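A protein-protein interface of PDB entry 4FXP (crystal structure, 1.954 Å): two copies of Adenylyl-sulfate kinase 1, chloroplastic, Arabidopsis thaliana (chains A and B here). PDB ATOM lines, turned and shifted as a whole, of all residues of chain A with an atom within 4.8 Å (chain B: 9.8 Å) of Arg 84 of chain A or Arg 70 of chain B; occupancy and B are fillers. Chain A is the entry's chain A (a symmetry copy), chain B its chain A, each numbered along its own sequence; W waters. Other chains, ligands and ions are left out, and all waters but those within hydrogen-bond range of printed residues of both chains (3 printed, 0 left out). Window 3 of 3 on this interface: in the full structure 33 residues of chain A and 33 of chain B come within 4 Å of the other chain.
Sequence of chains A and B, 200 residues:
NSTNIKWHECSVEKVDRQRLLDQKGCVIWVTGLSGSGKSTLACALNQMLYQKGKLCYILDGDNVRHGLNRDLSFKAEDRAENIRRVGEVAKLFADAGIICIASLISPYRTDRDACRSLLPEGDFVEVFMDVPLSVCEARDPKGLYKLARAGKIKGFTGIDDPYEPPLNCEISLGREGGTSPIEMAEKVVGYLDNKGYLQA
Arg 84 of chain A touches Arg 85 of chain B, and with the chains exchanged Arg 85 of chain A touches Arg 84 of chain B. Arg 85 of chain B touches its own counterpart, Arg 85 of chain A.
Of chain B, only Gly 67, Leu 68, Arg 70, Asp 71 and Arg 85 come within 4 Å of Arg 84 of chain A. Of chain A, only Arg 84 and Glu 88 come within 4 Å of Arg 70 of chain B. No residue of chain B comes within 4 Å of Gly 87 of chain A. Printed residues of chain A within 4 Å of Gly 67 of chain B: Arg 84 and Glu 88. Printed residues of chain A within 4 Å of Leu 68 of chain B: Arg 84, Arg 85 and Glu 88. Of the printed residues of chain A, Arg 84 of chain B touches Arg 85 (3.8 Å). Of the printed residues of chain A, Arg 85 of chain B touches Arg 84 (3.8 Å) and Arg 85 (3.4 Å). The nearest residue of chain A that does not touch Arg 70 of chain B is Leu 118 of chain A (4.1 Å). The nearest printed residue of chain A that does not touch Arg 85 of chain B is Glu 81 of chain A (4.03 Å).
The guanidinium group (NE) of Arg 70 of chain B is in hydrogen-bond range of the backbone carbonyl oxygen (O) of Gly 67 of chain B, at 3.2 Å. O of Leu 68 of chain B is in hydrogen-bond range of NH1 of Arg 85 of chain B, 3.3 Å away. The guanidinium group of Arg 85 of chain B is in hydrogen-bond range of the side-chain amide oxygen of Asn 69 of chain B, 3.0 Å away. The guanidinium group (NH1) of Arg 85 of chain B lies within salt-bridge range of the side-chain carboxylate (OD1) of Asp 71 of chain B (2.9 Å). OE2 of Glu 81 of chain B lies within salt-bridge range of NH2 of Arg 84 of chain B, 2.8 Å away. OE2 of Glu 81 of chain A is in salt-bridge range of NH2 of Arg 84 of chain A (2.8 Å).
Among the printed residues, merely in contact across the chains: Arg 85 of chain A with Leu 68 of chain B (3.6 Å), Glu 88 of chain A with Leu 68 of chain B (3.6 Å), Glu 81 of chain A with Asp 71 of chain B (3.8 Å), Arg 84 of chain A with Arg 85 of chain B (3.8 Å), Arg 85 of chain A with Arg 84 of chain B (3.8 Å) and Arg 84 of chain A with Arg 70 of chain B (3.9 Å).
O of Gly 67 of chain B is in hydrogen-bond range of NH1 of Arg 84 of chain A (3.3 Å). The backbone carbonyl oxygen (O) of Leu 68 of chain B is in hydrogen-bond range of the guanidinium group (NH2) of Arg 84 of chain A (2.8 Å). The side-chain carboxylate of Glu 88 of chain A lies within salt-bridge range of the guanidinium group of Arg 70 of chain B, at 2.8 Å. The side-chain carboxylate of Asp 71 of chain B lies within salt-bridge range of the guanidinium group of Arg 84 of chain A. NH2 of Arg 85 of chain B sits close to NH2 of Arg 85 of chain A (3.4 Å). O of Gly 67 of chain B sits close to OE2 of Glu 88 of chain A (3.4 Å).
Of the 20 printed residues of chain B, 6 touch a printed residue of chain A. Printed residues of chain B that touch a printed residue of chain A: Gly 67, Leu 68, Arg 70, Asp 71, Arg 84 and Arg 85. Hydrophobic or aromatic side chains of chain B that line the printed part of chain A: Leu 68. Along chain A the printed residues that touch a printed residue of chain B span positions 81 to 88. Among the printed residues, Asp or Glu carboxylates within 4 Å of a Lys or Arg side-chain nitrogen of the other chain: Arg 84 of chain A with Asp 71 of chain B (3.6 Å) and Glu 88 of chain A with Arg 70 of chain B (2.8 Å).
Water W2 lies within hydrogen-bond range of OE2 of Glu 88 of chain A (2.7 Å), NH1 of Arg 84 of chain A (2.9 Å) and NH1 of Arg 70 of chain B (3.2 Å). Water W1 lies within hydrogen-bond range of NH2 of Arg 85 of chain B, OE2 of Glu 81 of chain B and NH2 of Arg 85 of chain A. Water W3 lies within hydrogen-bond range of the guanidinium group of Arg 85 of chain A (2.9 Å), the side-chain carboxylate of Glu 81 of chain A (2.9 Å), the guanidinium group of Arg 85 of chain B (3.2 Å) and the side-chain carboxylate of Asp 71 of chain B (3.3 Å).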
ATOM      1  N   ALA A  80       9.098  14.487  -9.812  1.00  0.00           N
ATOM      2  CA  ALA A  80       9.139  14.996 -11.178  1.00  0.00           C
ATOM      3  C   ALA A  80      10.581  15.214 -11.635  1.00  0.00           C
ATOM      4  O   ALA A  80      10.947  14.826 -12.746  1.00  0.00           O
ATOM      5  CB  ALA A  80       8.330  16.278 -11.308  1.00  0.00           C
ATOM      6  N   GLU A  81      11.396  15.834 -10.780  1.00  0.00           N
ATOM      7  CA  GLU A  81      12.802  16.079 -11.114  1.00  0.00           C
ATOM      8  C   GLU A  81      13.581  14.762 -11.197  1.00  0.00           C
ATOM      9  O   GLU A  81      14.409  14.582 -12.090  1.00  0.00           O
ATOM     10  CB  GLU A  81      13.451  17.039 -10.105  1.00  0.00           C
ATOM     11  CG  GLU A  81      14.923  17.330 -10.358  1.00  0.00           C
ATOM     12  CD  GLU A  81      15.174  18.126 -11.632  1.00  0.00           C
ATOM     13  OE1 GLU A  81      14.200  18.511 -12.326  1.00  0.00           O
ATOM     14  OE2 GLU A  81      16.364  18.371 -11.936  1.00  0.00           O
ATOM     15  N   ASN A  82      13.298  13.844 -10.272  1.00  0.00           N
ATOM     16  CA  ASN A  82      13.896  12.503 -10.297  1.00  0.00           C
ATOM     17  C   ASN A  82      13.670  11.859 -11.665  1.00  0.00           C
ATOM     18  O   ASN A  82      14.607  11.401 -12.313  1.00  0.00           O
ATOM     19  CB  ASN A  82      13.253  11.626  -9.212  1.00  0.00           C
ATOM     20  CG  ASN A  82      13.900  10.251  -9.100  1.00  0.00           C
ATOM     21  OD1 ASN A  82      15.123  10.128  -9.039  1.00  0.00           O
ATOM     22  ND2 ASN A  82      13.076   9.212  -9.077  1.00  0.00           N
ATOM     23  N   ILE A  83      12.414  11.833 -12.089  1.00  0.00           N
ATOM     24  CA  ILE A  83      12.041  11.246 -13.370  1.00  0.00           C
ATOM     25  C   ILE A  83      12.653  11.988 -14.556  1.00  0.00           C
ATOM     26  O   ILE A  83      13.118  11.365 -15.513  1.00  0.00           O
ATOM     27  CB  ILE A  83      10.503  11.232 -13.546  1.00  0.00           C
ATOM     28  CG1 ILE A  83       9.856  10.295 -12.519  1.00  0.00           C
ATOM     29  CG2 ILE A  83      10.140  10.829 -14.968  1.00  0.00           C
ATOM     30  CD1 ILE A  83       8.395  10.648 -12.177  1.00  0.00           C
ATOM     31  N   ARG A  84      12.634  13.316 -14.501  1.00  0.00           N
ATOM     32  CA  ARG A  84      13.173  14.127 -15.583  1.00  0.00           C
ATOM     33  C   ARG A  84      14.661  13.845 -15.773  1.00  0.00           C
ATOM     34  O   ARG A  84      15.124  13.644 -16.892  1.00  0.00           O
ATOM     35  CB  ARG A  84      12.963  15.618 -15.316  1.00  0.00           C
ATOM     36  CG  ARG A  84      13.496  16.510 -16.439  1.00  0.00           C
ATOM     37  CD  ARG A  84      13.645  17.974 -15.998  1.00  0.00           C
ATOM     38  NE  ARG A  84      14.791  18.193 -15.114  1.00  0.00           N
ATOM     39  CZ  ARG A  84      16.042  18.377 -15.539  1.00  0.00           C
ATOM     40  NH1 ARG A  84      16.313  18.357 -16.836  1.00  0.00           N
ATOM     41  NH2 ARG A  84      17.030  18.575 -14.668  1.00  0.00           N
ATOM     42  N   ARG A  85      15.413  13.821 -14.679  1.00  0.00           N
ATOM     43  CA  ARG A  85      16.856  13.575 -14.790  1.00  0.00           C
ATOM     44  C   ARG A  85      17.136  12.165 -15.298  1.00  0.00           C
ATOM     45  O   ARG A  85      18.022  11.962 -16.134  1.00  0.00           O
ATOM     46  CB  ARG A  85      17.562  13.779 -13.450  1.00  0.00           C
ATOM     47  CG  ARG A  85      17.515  15.200 -12.892  1.00  0.00           C
ATOM     48  CD  ARG A  85      18.393  15.280 -11.635  1.00  0.00           C
ATOM     49  NE  ARG A  85      18.238  16.523 -10.879  1.00  0.00           N
ATOM     50  CZ  ARG A  85      18.699  16.700  -9.644  1.00  0.00           C
ATOM     51  NH1 ARG A  85      19.342  15.715  -9.028  1.00  0.00           N
ATOM     52  NH2 ARG A  85      18.507  17.853  -9.019  1.00  0.00           N
ATOM     53  N   VAL A  86      16.392  11.188 -14.790  1.00  0.00           N
ATOM     54  CA  VAL A  86      16.599   9.814 -15.231  1.00  0.00           C
ATOM     55  C   VAL A  86      16.298   9.713 -16.721  1.00  0.00           C
ATOM     56  O   VAL A  86      17.046   9.076 -17.466  1.00  0.00           O
ATOM     57  CB  VAL A  86      15.815   8.780 -14.399  1.00  0.00           C
ATOM     58  CG1 VAL A  86      15.882   7.413 -15.048  1.00  0.00           C
ATOM     59  CG2 VAL A  86      16.384   8.709 -12.980  1.00  0.00           C
ATOM     60  N   GLY A  87      15.235  10.381 -17.160  1.00  0.00           N
ATOM     61  CA  GLY A  87      14.901  10.428 -18.580  1.00  0.00           C
ATOM     62  C   GLY A  87      16.031  10.987 -19.437  1.00  0.00           C
ATOM     63  O   GLY A  87      16.342  10.460 -20.504  1.00  0.00           O
ATOM     64  N   GLU A  88      16.639  12.080 -18.989  1.00  0.00           N
ATOM     65  CA  GLU A  88      17.756  12.666 -19.727  1.00  0.00           C
ATOM     66  C   GLU A  88      18.975  11.731 -19.711  1.00  0.00           C
ATOM     67  O   GLU A  88      19.651  11.570 -20.724  1.00  0.00           O
ATOM     68  CB  GLU A  88      18.121  14.056 -19.181  1.00  0.00           C
ATOM     69  CG  GLU A  88      17.054  15.148 -19.386  1.00  0.00           C
ATOM     70  CD  GLU A  88      17.069  15.751 -20.789  1.00  0.00           C
ATOM     71  OE1 GLU A  88      17.761  15.220 -21.689  1.00  0.00           O
ATOM     72  OE2 GLU A  88      16.385  16.776 -20.991  1.00  0.00           O
ATOM     73  N   CYS A 115       9.539  12.121 -20.631  1.00  0.00           N
ATOM     74  CA  CYS A 115      10.725  11.321 -20.939  1.00  0.00           C
ATOM     75  C   CYS A 115      10.612  10.749 -22.336  1.00  0.00           C
ATOM     76  O   CYS A 115      11.576  10.742 -23.096  1.00  0.00           O
ATOM     77  CB  CYS A 115      10.900  10.188 -19.932  1.00  0.00           C
ATOM     78  SG  CYS A 115      11.307  10.770 -18.285  1.00  0.00           S
ATOM     79  N   LEU A 118      11.562  13.069 -25.157  1.00  0.00           N
ATOM     80  CA  LEU A 118      12.992  13.325 -25.338  1.00  0.00           C
ATOM     81  C   LEU A 118      13.608  12.466 -26.433  1.00  0.00           C
ATOM     82  O   LEU A 118      14.679  12.781 -26.944  1.00  0.00           O
ATOM     83  CB  LEU A 118      13.751  13.049 -24.039  1.00  0.00           C
ATOM     84  CG  LEU A 118      13.482  13.953 -22.842  1.00  0.00           C
ATOM     85  CD1 LEU A 118      14.263  13.446 -21.619  1.00  0.00           C
ATOM     86  CD2 LEU A 118      13.866  15.379 -23.186  1.00  0.00           C
ATOM     87  N   GLY B  61      30.079  19.789 -21.816  1.00  0.00           N
ATOM     88  CA  GLY B  61      29.439  20.767 -20.967  1.00  0.00           C
ATOM     89  C   GLY B  61      28.277  21.420 -21.663  1.00  0.00           C
ATOM     90  O   GLY B  61      27.164  21.422 -21.150  1.00  0.00           O
ATOM     91  N   ASP B  62      28.531  21.988 -22.833  1.00  0.00           N
ATOM     92  CA  ASP B  62      27.467  22.693 -23.523  1.00  0.00           C
ATOM     93  C   ASP B  62      26.278  21.765 -23.793  1.00  0.00           C
ATOM     94  O   ASP B  62      25.142  22.123 -23.482  1.00  0.00           O
ATOM     95  CB  ASP B  62      27.969  23.383 -24.797  1.00  0.00           C
ATOM     96  CG  ASP B  62      28.696  24.701 -24.504  1.00  0.00           C
ATOM     97  OD1 ASP B  62      29.951  24.718 -24.467  1.00  0.00           O
ATOM     98  OD2 ASP B  62      27.999  25.720 -24.299  1.00  0.00           O
ATOM     99  N   ASN B  63      26.523  20.586 -24.356  1.00  0.00           N
ATOM    100  CA  ASN B  63      25.397  19.684 -24.702  1.00  0.00           C
ATOM    101  C   ASN B  63      24.536  19.241 -23.520  1.00  0.00           C
ATOM    102  O   ASN B  63      23.313  19.401 -23.539  1.00  0.00           O
ATOM    103  CB  ASN B  63      25.875  18.450 -25.463  1.00  0.00           C
ATOM    104  CG  ASN B  63      26.592  18.800 -26.765  1.00  0.00           C
ATOM    105  OD1 ASN B  63      26.526  19.936 -27.245  1.00  0.00           O
ATOM    106  ND2 ASN B  63      27.283  17.815 -27.340  1.00  0.00           N
ATOM    107  N   VAL B  64      25.178  18.669 -22.505  1.00  0.00           N
ATOM    108  CA  VAL B  64      24.503  18.291 -21.270  1.00  0.00           C
ATOM    109  C   VAL B  64      23.713  19.466 -20.688  1.00  0.00           C
ATOM    110  O   VAL B  64      22.669  19.279 -20.069  1.00  0.00           O
ATOM    111  CB  VAL B  64      25.520  17.799 -20.218  1.00  0.00           C
ATOM    112  CG1 VAL B  64      24.825  17.506 -18.905  1.00  0.00           C
ATOM    113  CG2 VAL B  64      26.244  16.568 -20.722  1.00  0.00           C
ATOM    114  N   ARG B  65      24.213  20.681 -20.889  1.00  0.00           N
ATOM    115  CA  ARG B  65      23.520  21.865 -20.387  1.00  0.00           C
ATOM    116  C   ARG B  65      22.237  22.196 -21.149  1.00  0.00           C
ATOM    117  O   ARG B  65      21.467  23.059 -20.724  1.00  0.00           O
ATOM    118  CB  ARG B  65      24.446  23.086 -20.388  1.00  0.00           C
ATOM    119  CG  ARG B  65      25.333  23.185 -19.135  1.00  0.00           C
ATOM    120  CD  ARG B  65      26.234  24.404 -19.225  1.00  0.00           C
ATOM    121  NE  ARG B  65      26.973  24.659 -17.990  1.00  0.00           N
ATOM    122  CZ  ARG B  65      26.460  25.279 -16.929  1.00  0.00           C
ATOM    123  NH1 ARG B  65      25.198  25.689 -16.947  1.00  0.00           N
ATOM    124  NH2 ARG B  65      27.202  25.488 -15.846  1.00  0.00           N
ATOM    125  N   HIS B  66      22.004  21.535 -22.275  1.00  0.00           N
ATOM    126  CA  HIS B  66      20.710  21.698 -22.958  1.00  0.00           C
ATOM    127  C   HIS B  66      19.742  20.558 -22.670  1.00  0.00           C
ATOM    128  O   HIS B  66      18.630  20.534 -23.201  1.00  0.00           O
ATOM    129  CB  HIS B  66      20.890  21.881 -24.465  1.00  0.00           C
ATOM    130  CG  HIS B  66      21.691  23.095 -24.823  1.00  0.00           C
ATOM    131  ND1 HIS B  66      21.113  24.322 -25.071  1.00  0.00           N
ATOM    132  CD2 HIS B  66      23.025  23.276 -24.943  1.00  0.00           C
ATOM    133  CE1 HIS B  66      22.059  25.204 -25.341  1.00  0.00           C
ATOM    134  NE2 HIS B  66      23.230  24.597 -25.268  1.00  0.00           N
ATOM    135  N   GLY B  67      20.155  19.617 -21.824  1.00  0.00           N
ATOM    136  CA  GLY B  67      19.283  18.511 -21.472  1.00  0.00           C
ATOM    137  C   GLY B  67      19.178  18.293 -19.973  1.00  0.00           C
ATOM    138  O   GLY B  67      18.394  18.947 -19.293  1.00  0.00           O
ATOM    139  N   LEU B  68      19.976  17.368 -19.458  1.00  0.00           N
ATOM    140  CA  LEU B  68      19.974  17.064 -18.029  1.00  0.00           C
ATOM    141  C   LEU B  68      20.138  18.331 -17.183  1.00  0.00           C
ATOM    142  O   LEU B  68      19.421  18.531 -16.195  1.00  0.00           O
ATOM    143  CB  LEU B  68      21.093  16.078 -17.704  1.00  0.00           C
ATOM    144  CG  LEU B  68      21.313  15.781 -16.226  1.00  0.00           C
ATOM    145  CD1 LEU B  68      20.062  15.088 -15.646  1.00  0.00           C
ATOM    146  CD2 LEU B  68      22.545  14.914 -16.024  1.00  0.00           C
ATOM    147  N   ASN B  69      21.074  19.183 -17.585  1.00  0.00           N
ATOM    148  CA  ASN B  69      21.405  20.389 -16.816  1.00  0.00           C
ATOM    149  C   ASN B  69      20.833  21.688 -17.378  1.00  0.00           C
ATOM    150  O   ASN B  69      21.373  22.772 -17.151  1.00  0.00           O
ATOM    151  CB  ASN B  69      22.925  20.474 -16.593  1.00  0.00           C
ATOM    152  CG  ASN B  69      23.429  19.335 -15.724  1.00  0.00           C
ATOM    153  OD1 ASN B  69      22.623  18.614 -15.144  1.00  0.00           O
ATOM    154  ND2 ASN B  69      24.754  19.173 -15.622  1.00  0.00           N
ATOM    155  N   ARG B  70      19.707  21.571 -18.078  1.00  0.00           N
ATOM    156  CA  ARG B  70      19.062  22.734 -18.678  1.00  0.00           C
ATOM    157  C   ARG B  70      18.599  23.736 -17.622  1.00  0.00           C
ATOM    158  O   ARG B  70      18.349  24.899 -17.928  1.00  0.00           O
ATOM    159  CB  ARG B  70      17.875  22.308 -19.553  1.00  0.00           C
ATOM    160  CG  ARG B  70      16.720  21.741 -18.764  1.00  0.00           C
ATOM    161  CD  ARG B  70      15.559  21.338 -19.685  1.00  0.00           C
ATOM    162  NE  ARG B  70      16.001  20.455 -20.760  1.00  0.00           N
ATOM    163  CZ  ARG B  70      15.182  19.825 -21.598  1.00  0.00           C
ATOM    164  NH1 ARG B  70      13.867  19.979 -21.477  1.00  0.00           N
ATOM    165  NH2 ARG B  70      15.673  19.036 -22.548  1.00  0.00           N
ATOM    166  N   ASP B  71      18.480  23.281 -16.381  1.00  0.00           N
ATOM    167  CA  ASP B  71      18.020  24.144 -15.294  1.00  0.00           C
ATOM    168  C   ASP B  71      19.143  24.977 -14.650  1.00  0.00           C
ATOM    169  O   ASP B  71      18.881  25.835 -13.804  1.00  0.00           O
ATOM    170  CB  ASP B  71      17.286  23.312 -14.228  1.00  0.00           C
ATOM    171  CG  ASP B  71      18.127  22.147 -13.684  1.00  0.00           C
ATOM    172  OD1 ASP B  71      18.958  21.589 -14.432  1.00  0.00           O
ATOM    173  OD2 ASP B  71      17.940  21.782 -12.504  1.00  0.00           O
ATOM    174  N   LEU B  72      20.389  24.740 -15.054  1.00  0.00           N
ATOM    175  CA  LEU B  72      21.529  25.385 -14.393  1.00  0.00           C
ATOM    176  C   LEU B  72      22.091  26.628 -15.096  1.00  0.00           C
ATOM    177  O   LEU B  72      22.208  26.674 -16.323  1.00  0.00           O
ATOM    178  CB  LEU B  72      22.659  24.371 -14.175  1.00  0.00           C
ATOM    179  CG  LEU B  72      22.199  23.109 -13.447  1.00  0.00           C
ATOM    180  CD1 LEU B  72      23.358  22.113 -13.286  1.00  0.00           C
ATOM    181  CD2 LEU B  72      21.611  23.478 -12.098  1.00  0.00           C
ATOM    182  N   SER B  73      22.461  27.627 -14.300  1.00  0.00           N
ATOM    183  CA  SER B  73      23.108  28.826 -14.818  1.00  0.00           C
ATOM    184  C   SER B  73      24.614  28.731 -14.592  1.00  0.00           C
ATOM    185  O   SER B  73      25.143  27.647 -14.348  1.00  0.00           O
ATOM    186  CB  SER B  73      22.549  30.076 -14.137  1.00  0.00           C
ATOM    187  OG  SER B  73      22.964  30.150 -12.785  1.00  0.00           O
ATOM    188  N   PHE B  74      25.303  29.866 -14.672  1.00  0.00           N
ATOM    189  CA  PHE B  74      26.752  29.889 -14.443  1.00  0.00           C
ATOM    190  C   PHE B  74      27.206  30.518 -13.131  1.00  0.00           C
ATOM    191  O   PHE B  74      28.395  30.700 -12.889  1.00  0.00           O
ATOM    192  CB  PHE B  74      27.417  30.528 -15.670  1.00  0.00           C
ATOM    193  CG  PHE B  74      27.188  29.745 -16.929  1.00  0.00           C
ATOM    194  CD1 PHE B  74      28.078  28.761 -17.325  1.00  0.00           C
ATOM    195  CD2 PHE B  74      26.044  29.949 -17.682  1.00  0.00           C
ATOM    196  CE1 PHE B  74      27.847  28.014 -18.473  1.00  0.00           C
ATOM    197  CE2 PHE B  74      25.807  29.209 -18.831  1.00  0.00           C
ATOM    198  CZ  PHE B  74      26.702  28.241 -19.226  1.00  0.00           C
ATOM    199  N   ASP B  78      25.783  26.895  -9.300  1.00  0.00           N
ATOM    200  CA  ASP B  78      25.194  26.134 -10.402  1.00  0.00           C
ATOM    201  C   ASP B  78      26.280  25.403 -11.180  1.00  0.00           C
ATOM    202  O   ASP B  78      26.051  24.314 -11.702  1.00  0.00           O
ATOM    203  CB  ASP B  78      24.378  27.037 -11.328  1.00  0.00           C
ATOM    204  CG  ASP B  78      22.932  27.186 -10.870  1.00  0.00           C
ATOM    205  OD1 ASP B  78      22.647  26.889  -9.691  1.00  0.00           O
ATOM    206  OD2 ASP B  78      22.079  27.596 -11.684  1.00  0.00           O
ATOM    207  N   GLU B  81      26.916  22.319  -9.167  1.00  0.00           N
ATOM    208  CA  GLU B  81      25.896  21.299  -9.427  1.00  0.00           C
ATOM    209  C   GLU B  81      26.075  20.690 -10.821  1.00  0.00           C
ATOM    210  O   GLU B  81      25.940  19.479 -10.995  1.00  0.00           O
ATOM    211  CB  GLU B  81      24.482  21.877  -9.256  1.00  0.00           C
ATOM    212  CG  GLU B  81      23.354  20.893  -9.534  1.00  0.00           C
ATOM    213  CD  GLU B  81      23.269  19.764  -8.516  1.00  0.00           C
ATOM    214  OE1 GLU B  81      24.060  19.747  -7.541  1.00  0.00           O
ATOM    215  OE2 GLU B  81      22.394  18.887  -8.697  1.00  0.00           O
ATOM    216  N   ASN B  82      26.395  21.534 -11.803  1.00  0.00           N
ATOM    217  CA  ASN B  82      26.696  21.069 -13.162  1.00  0.00           C
ATOM    218  C   ASN B  82      27.778  19.992 -13.115  1.00  0.00           C
ATOM    219  O   ASN B  82      27.612  18.900 -13.655  1.00  0.00           O
ATOM    220  CB  ASN B  82      27.189  22.246 -14.018  1.00  0.00           C
ATOM    221  CG  ASN B  82      27.416  21.866 -15.476  1.00  0.00           C
ATOM    222  OD1 ASN B  82      26.563  21.243 -16.109  1.00  0.00           O
ATOM    223  ND2 ASN B  82      28.571  22.239 -16.009  1.00  0.00           N
ATOM    224  N   ARG B  84      28.923  18.313 -10.449  1.00  0.00           N
ATOM    225  CA  ARG B  84      28.540  17.190  -9.607  1.00  0.00           C
ATOM    226  C   ARG B  84      27.686  16.199 -10.393  1.00  0.00           C
ATOM    227  O   ARG B  84      27.922  14.995 -10.351  1.00  0.00           O
ATOM    228  CB  ARG B  84      27.775  17.659  -8.370  1.00  0.00           C
ATOM    229  CG  ARG B  84      27.369  16.512  -7.442  1.00  0.00           C
ATOM    230  CD  ARG B  84      26.283  16.931  -6.439  1.00  0.00           C
ATOM    231  NE  ARG B  84      24.960  17.068  -7.050  1.00  0.00           N
ATOM    232  CZ  ARG B  84      24.123  16.051  -7.264  1.00  0.00           C
ATOM    233  NH1 ARG B  84      24.476  14.818  -6.928  1.00  0.00           N
ATOM    234  NH2 ARG B  84      22.932  16.262  -7.822  1.00  0.00           N
ATOM    235  N   ARG B  85      26.695  16.703 -11.119  1.00  0.00           N
ATOM    236  CA  ARG B  85      25.821  15.806 -11.883  1.00  0.00           C
ATOM    237  C   ARG B  85      26.591  15.104 -12.996  1.00  0.00           C
ATOM    238  O   ARG B  85      26.402  13.908 -13.234  1.00  0.00           O
ATOM    239  CB  ARG B  85      24.637  16.561 -12.488  1.00  0.00           C
ATOM    240  CG  ARG B  85      23.669  17.181 -11.482  1.00  0.00           C
ATOM    241  CD  ARG B  85      22.462  17.762 -12.231  1.00  0.00           C
ATOM    242  NE  ARG B  85      21.587  18.589 -11.400  1.00  0.00           N
ATOM    243  CZ  ARG B  85      20.641  19.387 -11.887  1.00  0.00           C
ATOM    244  NH1 ARG B  85      20.449  19.464 -13.198  1.00  0.00           N
ATOM    245  NH2 ARG B  85      19.896  20.116 -11.068  1.00  0.00           N
ATOM    246  N   VAL B  86      27.453  15.845 -13.685  1.00  0.00           N
ATOM    247  CA  VAL B  86      28.230  15.241 -14.761  1.00  0.00           C
ATOM    248  C   VAL B  86      29.124  14.150 -14.186  1.00  0.00           C
ATOM    249  O   VAL B  86      29.233  13.065 -14.761  1.00  0.00           O
ATOM    250  CB  VAL B  86      29.017  16.269 -15.598  1.00  0.00           C
ATOM    251  CG1 VAL B  86      29.979  15.568 -16.535  1.00  0.00           C
ATOM    252  CG2 VAL B  86      28.050  17.139 -16.404  1.00  0.00           C
HETATM  253  O   HOH W   1      20.035  20.543  -8.175  1.00  0.00           O
HETATM  254  O   HOH W   2      14.720  17.831 -19.203  1.00  0.00           O
HETATM  255  O   HOH W   3      16.972  20.234  -9.759  1.00  0.00           O
